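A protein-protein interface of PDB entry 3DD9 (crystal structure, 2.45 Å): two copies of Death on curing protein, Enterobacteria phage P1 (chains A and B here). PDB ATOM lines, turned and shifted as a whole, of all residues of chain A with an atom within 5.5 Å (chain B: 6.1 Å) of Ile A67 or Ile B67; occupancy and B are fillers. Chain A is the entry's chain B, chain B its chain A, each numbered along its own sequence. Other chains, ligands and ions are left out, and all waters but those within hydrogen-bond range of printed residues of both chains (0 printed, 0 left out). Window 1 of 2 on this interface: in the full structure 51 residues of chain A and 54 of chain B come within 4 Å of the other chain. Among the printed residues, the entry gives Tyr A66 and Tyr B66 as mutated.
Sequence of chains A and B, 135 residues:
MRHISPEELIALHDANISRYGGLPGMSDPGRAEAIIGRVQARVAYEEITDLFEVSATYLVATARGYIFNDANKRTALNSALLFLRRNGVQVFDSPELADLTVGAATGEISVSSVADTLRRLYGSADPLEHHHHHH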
ATOM      1  N   ARG A  31      14.582   3.616  15.375  1.00  0.00           N
ATOM      2  CA  ARG A  31      13.700   2.727  14.667  1.00  0.00           C
ATOM      3  C   ARG A  31      12.564   3.532  14.043  1.00  0.00           C
ATOM      4  O   ARG A  31      12.243   3.384  12.893  1.00  0.00           O
ATOM      5  CB  ARG A  31      13.164   1.710  15.662  1.00  0.00           C
ATOM      6  CG  ARG A  31      12.569   0.490  15.084  1.00  0.00           C
ATOM      7  CD  ARG A  31      13.602  -0.343  14.437  1.00  0.00           C
ATOM      8  NE  ARG A  31      14.138  -1.376  15.303  1.00  0.00           N
ATOM      9  CZ  ARG A  31      14.071  -2.667  15.040  1.00  0.00           C
ATOM     10  NH1 ARG A  31      13.455  -3.072  13.969  1.00  0.00           N
ATOM     11  NH2 ARG A  31      14.600  -3.550  15.852  1.00  0.00           N
ATOM     12  N   ALA A  63       4.632  -1.938   9.924  1.00  0.00           N
ATOM     13  CA  ALA A  63       4.665  -3.380  10.145  1.00  0.00           C
ATOM     14  C   ALA A  63       6.095  -3.967   9.954  1.00  0.00           C
ATOM     15  O   ALA A  63       6.626  -4.605  10.875  1.00  0.00           O
ATOM     16  CB  ALA A  63       3.683  -4.040   9.244  1.00  0.00           C
ATOM     17  N   ARG A  64       6.722  -3.728   8.785  1.00  0.00           N
ATOM     18  CA  ARG A  64       8.065  -4.279   8.452  1.00  0.00           C
ATOM     19  C   ARG A  64       9.162  -3.732   9.338  1.00  0.00           C
ATOM     20  O   ARG A  64      10.221  -4.325   9.483  1.00  0.00           O
ATOM     21  CB  ARG A  64       8.391  -4.135   6.980  1.00  0.00           C
ATOM     22  CG  ARG A  64       7.240  -4.601   6.173  1.00  0.00           C
ATOM     23  CD  ARG A  64       7.642  -4.995   4.854  1.00  0.00           C
ATOM     24  NE  ARG A  64       6.533  -5.693   4.241  1.00  0.00           N
ATOM     25  CZ  ARG A  64       6.343  -5.726   2.929  1.00  0.00           C
ATOM     26  NH1 ARG A  64       7.198  -5.092   2.134  1.00  0.00           N
ATOM     27  NH2 ARG A  64       5.315  -6.396   2.423  1.00  0.00           N
ATOM     28  N   GLY A  65       8.894  -2.576   9.913  1.00  0.00           N
ATOM     29  CA  GLY A  65       8.832  -2.563  11.385  1.00  0.00           C
ATOM     30  C   GLY A  65      10.062  -2.071  11.993  1.00  0.00           C
ATOM     31  O   GLY A  65      10.841  -1.501  11.276  1.00  0.00           O
ATOM     32  N   TYR A  66      10.257  -2.276  13.286  1.00  0.00           N
ATOM     33  CA  TYR A  66       9.390  -3.095  14.217  1.00  0.00           C
ATOM     34  C   TYR A  66       9.397  -4.618  14.131  1.00  0.00           C
ATOM     35  O   TYR A  66       8.812  -5.288  14.978  1.00  0.00           O
ATOM     36  CB  TYR A  66       7.986  -2.523  14.496  1.00  0.00           C
ATOM     37  CG  TYR A  66       8.065  -1.136  15.076  1.00  0.00           C
ATOM     38  CD1 TYR A  66       9.019  -0.824  16.058  1.00  0.00           C
ATOM     39  CD2 TYR A  66       7.211  -0.134  14.646  1.00  0.00           C
ATOM     40  CE1 TYR A  66       9.111   0.453  16.590  1.00  0.00           C
ATOM     41  CE2 TYR A  66       7.300   1.128  15.166  1.00  0.00           C
ATOM     42  CZ  TYR A  66       8.261   1.417  16.119  1.00  0.00           C
ATOM     43  OH  TYR A  66       8.333   2.678  16.614  1.00  0.00           O
ATOM     44  N   ILE A  67      10.073  -5.169  13.139  1.00  0.00           N
ATOM     45  CA  ILE A  67      10.460  -6.566  13.202  1.00  0.00           C
ATOM     46  C   ILE A  67      11.746  -6.623  14.033  1.00  0.00           C
ATOM     47  O   ILE A  67      12.769  -6.021  13.690  1.00  0.00           O
ATOM     48  CB  ILE A  67      10.631  -7.154  11.804  1.00  0.00           C
ATOM     49  CG1 ILE A  67       9.261  -7.232  11.123  1.00  0.00           C
ATOM     50  CG2 ILE A  67      11.307  -8.500  11.872  1.00  0.00           C
ATOM     51  CD1 ILE A  67       9.335  -7.528   9.640  1.00  0.00           C
ATOM     52  N   PHE A  68      11.676  -7.296  15.166  1.00  0.00           N
ATOM     53  CA  PHE A  68      12.839  -7.371  16.041  1.00  0.00           C
ATOM     54  C   PHE A  68      13.566  -8.700  15.883  1.00  0.00           C
ATOM     55  O   PHE A  68      12.964  -9.721  15.462  1.00  0.00           O
ATOM     56  CB  PHE A  68      12.439  -7.138  17.496  1.00  0.00           C
ATOM     57  CG  PHE A  68      12.020  -5.719  17.794  1.00  0.00           C
ATOM     58  CD1 PHE A  68      12.969  -4.704  17.898  1.00  0.00           C
ATOM     59  CD2 PHE A  68      10.677  -5.395  17.974  1.00  0.00           C
ATOM     60  CE1 PHE A  68      12.590  -3.370  18.190  1.00  0.00           C
ATOM     61  CE2 PHE A  68      10.282  -4.067  18.262  1.00  0.00           C
ATOM     62  CZ  PHE A  68      11.246  -3.060  18.373  1.00  0.00           C
ATOM     63  N   ASN A  69      14.867  -8.682  16.163  1.00  0.00           N
ATOM     64  CA  ASN A  69      15.614  -9.921  16.340  1.00  0.00           C
ATOM     65  C   ASN A  69      15.281 -10.454  17.736  1.00  0.00           C
ATOM     66  O   ASN A  69      16.044 -10.299  18.672  1.00  0.00           O
ATOM     67  CB  ASN A  69      17.126  -9.710  16.124  1.00  0.00           C
ATOM     68  CG  ASN A  69      17.932 -11.004  16.237  1.00  0.00           C
ATOM     69  OD1 ASN A  69      19.098 -10.990  16.662  1.00  0.00           O
ATOM     70  ND2 ASN A  69      17.311 -12.133  15.878  1.00  0.00           N
ATOM     71  N   ASN A  72      10.070 -14.165  18.515  1.00  0.00           N
ATOM     72  CA  ASN A  72       9.172 -14.492  17.443  1.00  0.00           C
ATOM     73  C   ASN A  72       9.938 -14.792  16.184  1.00  0.00           C
ATOM     74  O   ASN A  72       9.546 -15.673  15.422  1.00  0.00           O
ATOM     75  CB  ASN A  72       8.193 -13.353  17.193  1.00  0.00           C
ATOM     76  CG  ASN A  72       7.378 -13.006  18.431  1.00  0.00           C
ATOM     77  OD1 ASN A  72       6.669 -13.858  18.987  1.00  0.00           O
ATOM     78  ND2 ASN A  72       7.461 -11.737  18.861  1.00  0.00           N
ATOM     79  N   LYS A  73      11.041 -14.080  15.969  1.00  0.00           N
ATOM     80  CA  LYS A  73      11.834 -14.330  14.770  1.00  0.00           C
ATOM     81  C   LYS A  73      12.532 -15.686  14.861  1.00  0.00           C
ATOM     82  O   LYS A  73      12.642 -16.394  13.862  1.00  0.00           O
ATOM     83  CB  LYS A  73      12.869 -13.232  14.572  1.00  0.00           C
ATOM     84  CG  LYS A  73      13.313 -13.080  13.158  1.00  0.00           C
ATOM     85  CD  LYS A  73      14.358 -11.995  13.056  1.00  0.00           C
ATOM     86  CE  LYS A  73      15.723 -12.594  12.775  1.00  0.00           C
ATOM     87  NZ  LYS A  73      16.507 -11.679  11.879  1.00  0.00           N
ATOM     88  N   ALA A  76      10.379 -18.967  14.336  1.00  0.00           N
ATOM     89  CA  ALA A  76      10.069 -19.277  12.939  1.00  0.00           C
ATOM     90  C   ALA A  76      11.193 -20.119  12.393  1.00  0.00           C
ATOM     91  O   ALA A  76      10.976 -21.169  11.795  1.00  0.00           O
ATOM     92  CB  ALA A  76       9.908 -18.002  12.116  1.00  0.00           C
ATOM     93  N   THR A 101      14.588 -15.073   7.278  1.00  0.00           N
ATOM     94  CA  THR A 101      13.338 -15.093   8.034  1.00  0.00           C
ATOM     95  C   THR A 101      12.457 -13.885   7.789  1.00  0.00           C
ATOM     96  O   THR A 101      11.247 -14.038   7.471  1.00  0.00           O
ATOM     97  CB  THR A 101      13.604 -15.240   9.538  1.00  0.00           C
ATOM     98  OG1 THR A 101      14.234 -16.485   9.735  1.00  0.00           O
ATOM     99  CG2 THR A 101      12.330 -15.285  10.309  1.00  0.00           C
ATOM    100  N   VAL A 102      13.073 -12.707   7.921  1.00  0.00           N
ATOM    101  CA  VAL A 102      12.431 -11.416   7.726  1.00  0.00           C
ATOM    102  C   VAL A 102      11.929 -11.354   6.297  1.00  0.00           C
ATOM    103  O   VAL A 102      10.748 -11.097   6.068  1.00  0.00           O
ATOM    104  CB  VAL A 102      13.431 -10.242   7.990  1.00  0.00           C
ATOM    105  CG1 VAL A 102      12.815  -8.873   7.659  1.00  0.00           C
ATOM    106  CG2 VAL A 102      13.931 -10.283   9.419  1.00  0.00           C
ATOM    107  N   ALA A 105       9.019 -13.576   5.935  1.00  0.00           N
ATOM    108  CA  ALA A 105       7.846 -13.000   6.557  1.00  0.00           C
ATOM    109  C   ALA A 105       7.216 -11.906   5.686  1.00  0.00           C
ATOM    110  O   ALA A 105       5.993 -11.792   5.634  1.00  0.00           O
ATOM    111  CB  ALA A 105       8.187 -12.450   7.985  1.00  0.00           C
ATOM    112  N   THR A 106       8.044 -11.107   5.017  1.00  0.00           N
ATOM    113  CA  THR A 106       7.559  -9.908   4.328  1.00  0.00           C
ATOM    114  C   THR A 106       7.191 -10.165   2.887  1.00  0.00           C
ATOM    115  O   THR A 106       6.761  -9.240   2.190  1.00  0.00           O
ATOM    116  CB  THR A 106       8.598  -8.752   4.315  1.00  0.00           C
ATOM    117  OG1 THR A 106       9.790  -9.207   3.669  1.00  0.00           O
ATOM    118  CG2 THR A 106       8.927  -8.270   5.713  1.00  0.00           C
ATOM    119  N   THR B  62       5.330 -19.739  10.139  1.00  0.00           N
ATOM    120  CA  THR B  62       5.611 -19.497  11.535  1.00  0.00           C
ATOM    121  C   THR B  62       6.028 -18.021  11.661  1.00  0.00           C
ATOM    122  O   THR B  62       5.641 -17.336  12.590  1.00  0.00           O
ATOM    123  CB  THR B  62       6.665 -20.508  12.068  1.00  0.00           C
ATOM    124  OG1 THR B  62       6.182 -21.834  11.847  1.00  0.00           O
ATOM    125  CG2 THR B  62       6.876 -20.347  13.536  1.00  0.00           C
ATOM    126  N   ALA B  63       6.749 -17.526  10.669  1.00  0.00           N
ATOM    127  CA  ALA B  63       7.247 -16.163  10.707  1.00  0.00           C
ATOM    128  C   ALA B  63       6.078 -15.169  10.700  1.00  0.00           C
ATOM    129  O   ALA B  63       6.016 -14.264  11.516  1.00  0.00           O
ATOM    130  CB  ALA B  63       8.242 -15.913   9.535  1.00  0.00           C
ATOM    131  N   ARG B  64       5.140 -15.395   9.795  1.00  0.00           N
ATOM    132  CA  ARG B  64       3.955 -14.580   9.662  1.00  0.00           C
ATOM    133  C   ARG B  64       3.076 -14.555  10.879  1.00  0.00           C
ATOM    134  O   ARG B  64       2.517 -13.511  11.228  1.00  0.00           O
ATOM    135  CB  ARG B  64       3.140 -15.023   8.452  1.00  0.00           C
ATOM    136  CG  ARG B  64       3.727 -14.471   7.203  1.00  0.00           C
ATOM    137  CD  ARG B  64       3.285 -15.128   5.917  1.00  0.00           C
ATOM    138  NE  ARG B  64       4.158 -14.512   4.927  1.00  0.00           N
ATOM    139  CZ  ARG B  64       4.053 -14.598   3.608  1.00  0.00           C
ATOM    140  NH1 ARG B  64       3.069 -15.297   3.023  1.00  0.00           N
ATOM    141  NH2 ARG B  64       4.961 -13.951   2.885  1.00  0.00           N
ATOM    142  N   GLY B  65       2.941 -15.682  11.529  1.00  0.00           N
ATOM    143  CA  GLY B  65       2.008 -15.716  12.640  1.00  0.00           C
ATOM    144  C   GLY B  65       2.632 -15.235  13.935  1.00  0.00           C
ATOM    145  O   GLY B  65       1.899 -14.773  14.813  1.00  0.00           O
ATOM    146  N   TYR B  66       3.923 -15.328  14.073  1.00  0.00           N
ATOM    147  CA  TYR B  66       4.536 -14.851  15.297  1.00  0.00           C
ATOM    148  C   TYR B  66       5.043 -13.434  15.160  1.00  0.00           C
ATOM    149  O   TYR B  66       4.858 -12.614  16.050  1.00  0.00           O
ATOM    150  CB  TYR B  66       5.628 -15.809  15.771  1.00  0.00           C
ATOM    151  CG  TYR B  66       5.064 -17.040  16.456  1.00  0.00           C
ATOM    152  CD1 TYR B  66       4.737 -17.020  17.810  1.00  0.00           C
ATOM    153  CD2 TYR B  66       4.850 -18.211  15.751  1.00  0.00           C
ATOM    154  CE1 TYR B  66       4.230 -18.160  18.459  1.00  0.00           C
ATOM    155  CE2 TYR B  66       4.334 -19.351  16.374  1.00  0.00           C
ATOM    156  CZ  TYR B  66       4.017 -19.318  17.726  1.00  0.00           C
ATOM    157  OH  TYR B  66       3.514 -20.444  18.344  1.00  0.00           O
ATOM    158  N   ILE B  67       5.655 -13.120  14.027  1.00  0.00           N
ATOM    159  CA  ILE B  67       6.239 -11.812  13.890  1.00  0.00           C
ATOM    160  C   ILE B  67       5.147 -10.736  13.763  1.00  0.00           C
ATOM    161  O   ILE B  67       5.191  -9.717  14.459  1.00  0.00           O
ATOM    162  CB  ILE B  67       7.277 -11.765  12.728  1.00  0.00           C
ATOM    163  CG1 ILE B  67       8.494 -12.643  13.056  1.00  0.00           C
ATOM    164  CG2 ILE B  67       7.689 -10.300  12.424  1.00  0.00           C
ATOM    165  CD1 ILE B  67       9.541 -12.705  11.949  1.00  0.00           C
ATOM    166  N   PHE B  68       4.164 -10.945  12.891  1.00  0.00           N
ATOM    167  CA  PHE B  68       3.075  -9.978  12.819  1.00  0.00           C
ATOM    168  C   PHE B  68       2.014 -10.293  13.843  1.00  0.00           C
ATOM    169  O   PHE B  68       0.871 -10.636  13.515  1.00  0.00           O
ATOM    170  CB  PHE B  68       2.512  -9.850  11.406  1.00  0.00           C
ATOM    171  CG  PHE B  68       3.554  -9.605  10.398  1.00  0.00           C
ATOM    172  CD1 PHE B  68       4.327  -8.450  10.463  1.00  0.00           C
ATOM    173  CD2 PHE B  68       3.848 -10.568   9.441  1.00  0.00           C
ATOM    174  CE1 PHE B  68       5.346  -8.229   9.543  1.00  0.00           C
ATOM    175  CE2 PHE B  68       4.873 -10.365   8.534  1.00  0.00           C
ATOM    176  CZ  PHE B  68       5.617  -9.176   8.577  1.00  0.00           C
ATOM    177  N   ASN B  69       2.428 -10.172  15.094  1.00  0.00           N
ATOM    178  CA  ASN B  69       1.571 -10.341  16.241  1.00  0.00           C
ATOM    179  C   ASN B  69       0.686  -9.114  16.454  1.00  0.00           C
ATOM    180  O   ASN B  69       0.727  -8.169  15.679  1.00  0.00           O
ATOM    181  CB  ASN B  69       2.441 -10.574  17.484  1.00  0.00           C
ATOM    182  CG  ASN B  69       3.449  -9.427  17.723  1.00  0.00           C
ATOM    183  OD1 ASN B  69       3.080  -8.260  17.758  1.00  0.00           O
ATOM    184  ND2 ASN B  69       4.709  -9.774  17.887  1.00  0.00           N
ATOM    185  N   ASN B  72       2.360  -5.583  16.915  1.00  0.00           N
ATOM    186  CA  ASN B  72       2.866  -5.127  15.656  1.00  0.00           C
ATOM    187  C   ASN B  72       1.745  -4.670  14.723  1.00  0.00           C
ATOM    188  O   ASN B  72       1.802  -3.607  14.192  1.00  0.00           O
ATOM    189  CB  ASN B  72       3.717  -6.221  15.035  1.00  0.00           C
ATOM    190  CG  ASN B  72       4.233  -5.865  13.681  1.00  0.00           C
ATOM    191  OD1 ASN B  72       3.523  -5.927  12.710  1.00  0.00           O
ATOM    192  ND2 ASN B  72       5.472  -5.487  13.615  1.00  0.00           N
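NE of Arg B64 lies within hydrogen-bond range of O of Ala A105, at 3.4 Å. The backbone carbonyl oxygen (O) of Ala A63 lies within hydrogen-bond range of the side-chain amide nitrogen (ND2) of Asn B72 (3.1 Å).
O of Tyr B66 lies within hydrogen-bond range of ND2 of Asn B69, at 3.4 Å. The backbone carbonyl oxygen of Ile B67 is in hydrogen-bond range of the side-chain amide nitrogen of Asn B69. The side-chain amide oxygen (OD1) of Asn B69 sits at hydrogen-bond distance from the backbone NH (N) of Asn B72, 2.9 Å away. NH1 of Arg A31 is in hydrogen-bond range of O of Ile A67 (3.0 Å).
Among the printed residues, pairs that only touch across the chains: Tyr A66 with Asn B72 (3.6 Å), Ile A67 with Ile B67 (3.7 Å), Asn A72 with Tyr B66 (3.5 Å), Asn A72 with Ile B67 (3.99 Å), Asn A72 with Asn B69 (3.5 Å), Lys A73 with Ile B67 (3.98 Å), Ala A76 with Thr B62 (3.4 Å), Ala A76 with Ala B63 (3.5 Å), Ala A105 with Ala B63 (3.8 Å) and Ala A105 with Phe B68 (3.4 Å).
Arg A64 touches none of the printed residues of chain B. Of chain B, only Ile B67 comes within 4 Å of Ile A67. Printed residues of chain B within 4 Å of Lys A73: Ile B67. Of the printed residues of chain B, Ala A76 touches Thr B62 and Ala B63. Printed residues of chain A within 4 Å of Thr B62: Ala A76. Of the printed residues of chain A, Ile B67 touches Ile A67, Asn A72 and Lys A73. The nearest residue of chain B that does not touch Ile A67 is Phe B68 (4.1 Å). The nearest printed residue of chain B that does not touch Asn A72 is Thr B62 (5.1 Å).
Of the 15 printed residues of chain A, 7 touch a printed residue of chain B. Hydrophobic or aromatic side chains of chain A within 4 Å of the printed part of chain B: Ala A63, Tyr A66, Ile A67, Ala A76 and Ala A105. Hydrophobic or aromatic side chains of chain B that line the printed part of chain A: Ala B63, Tyr B66, Ile B67 and Phe B68. Among the printed residues, 12 pairs touch across the chains. Among the printed residues, no Asp or Glu carboxylate lies within 4 Å of a Lys or Arg side-chain nitrogen of the other chain.
Ala A63 touches Asn B72, but with the chains exchanged Asn A72 does not touch Ala B63 (5.3 Å). Tyr A66 touches Asn B72, and with the chains exchanged Asn A72 touches Tyr B66. Ile B67 touches its own counterpart, Ile A67. Asn A72 touches Ile B67, but with the chains exchanged Ile A67 does not touch Asn B72 (4.6 Å). 8 positions are printed for both chains. Of the 12 pairs that touch across the chains among the printed residues, 3 have their exchanged pair printed and touching as well.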
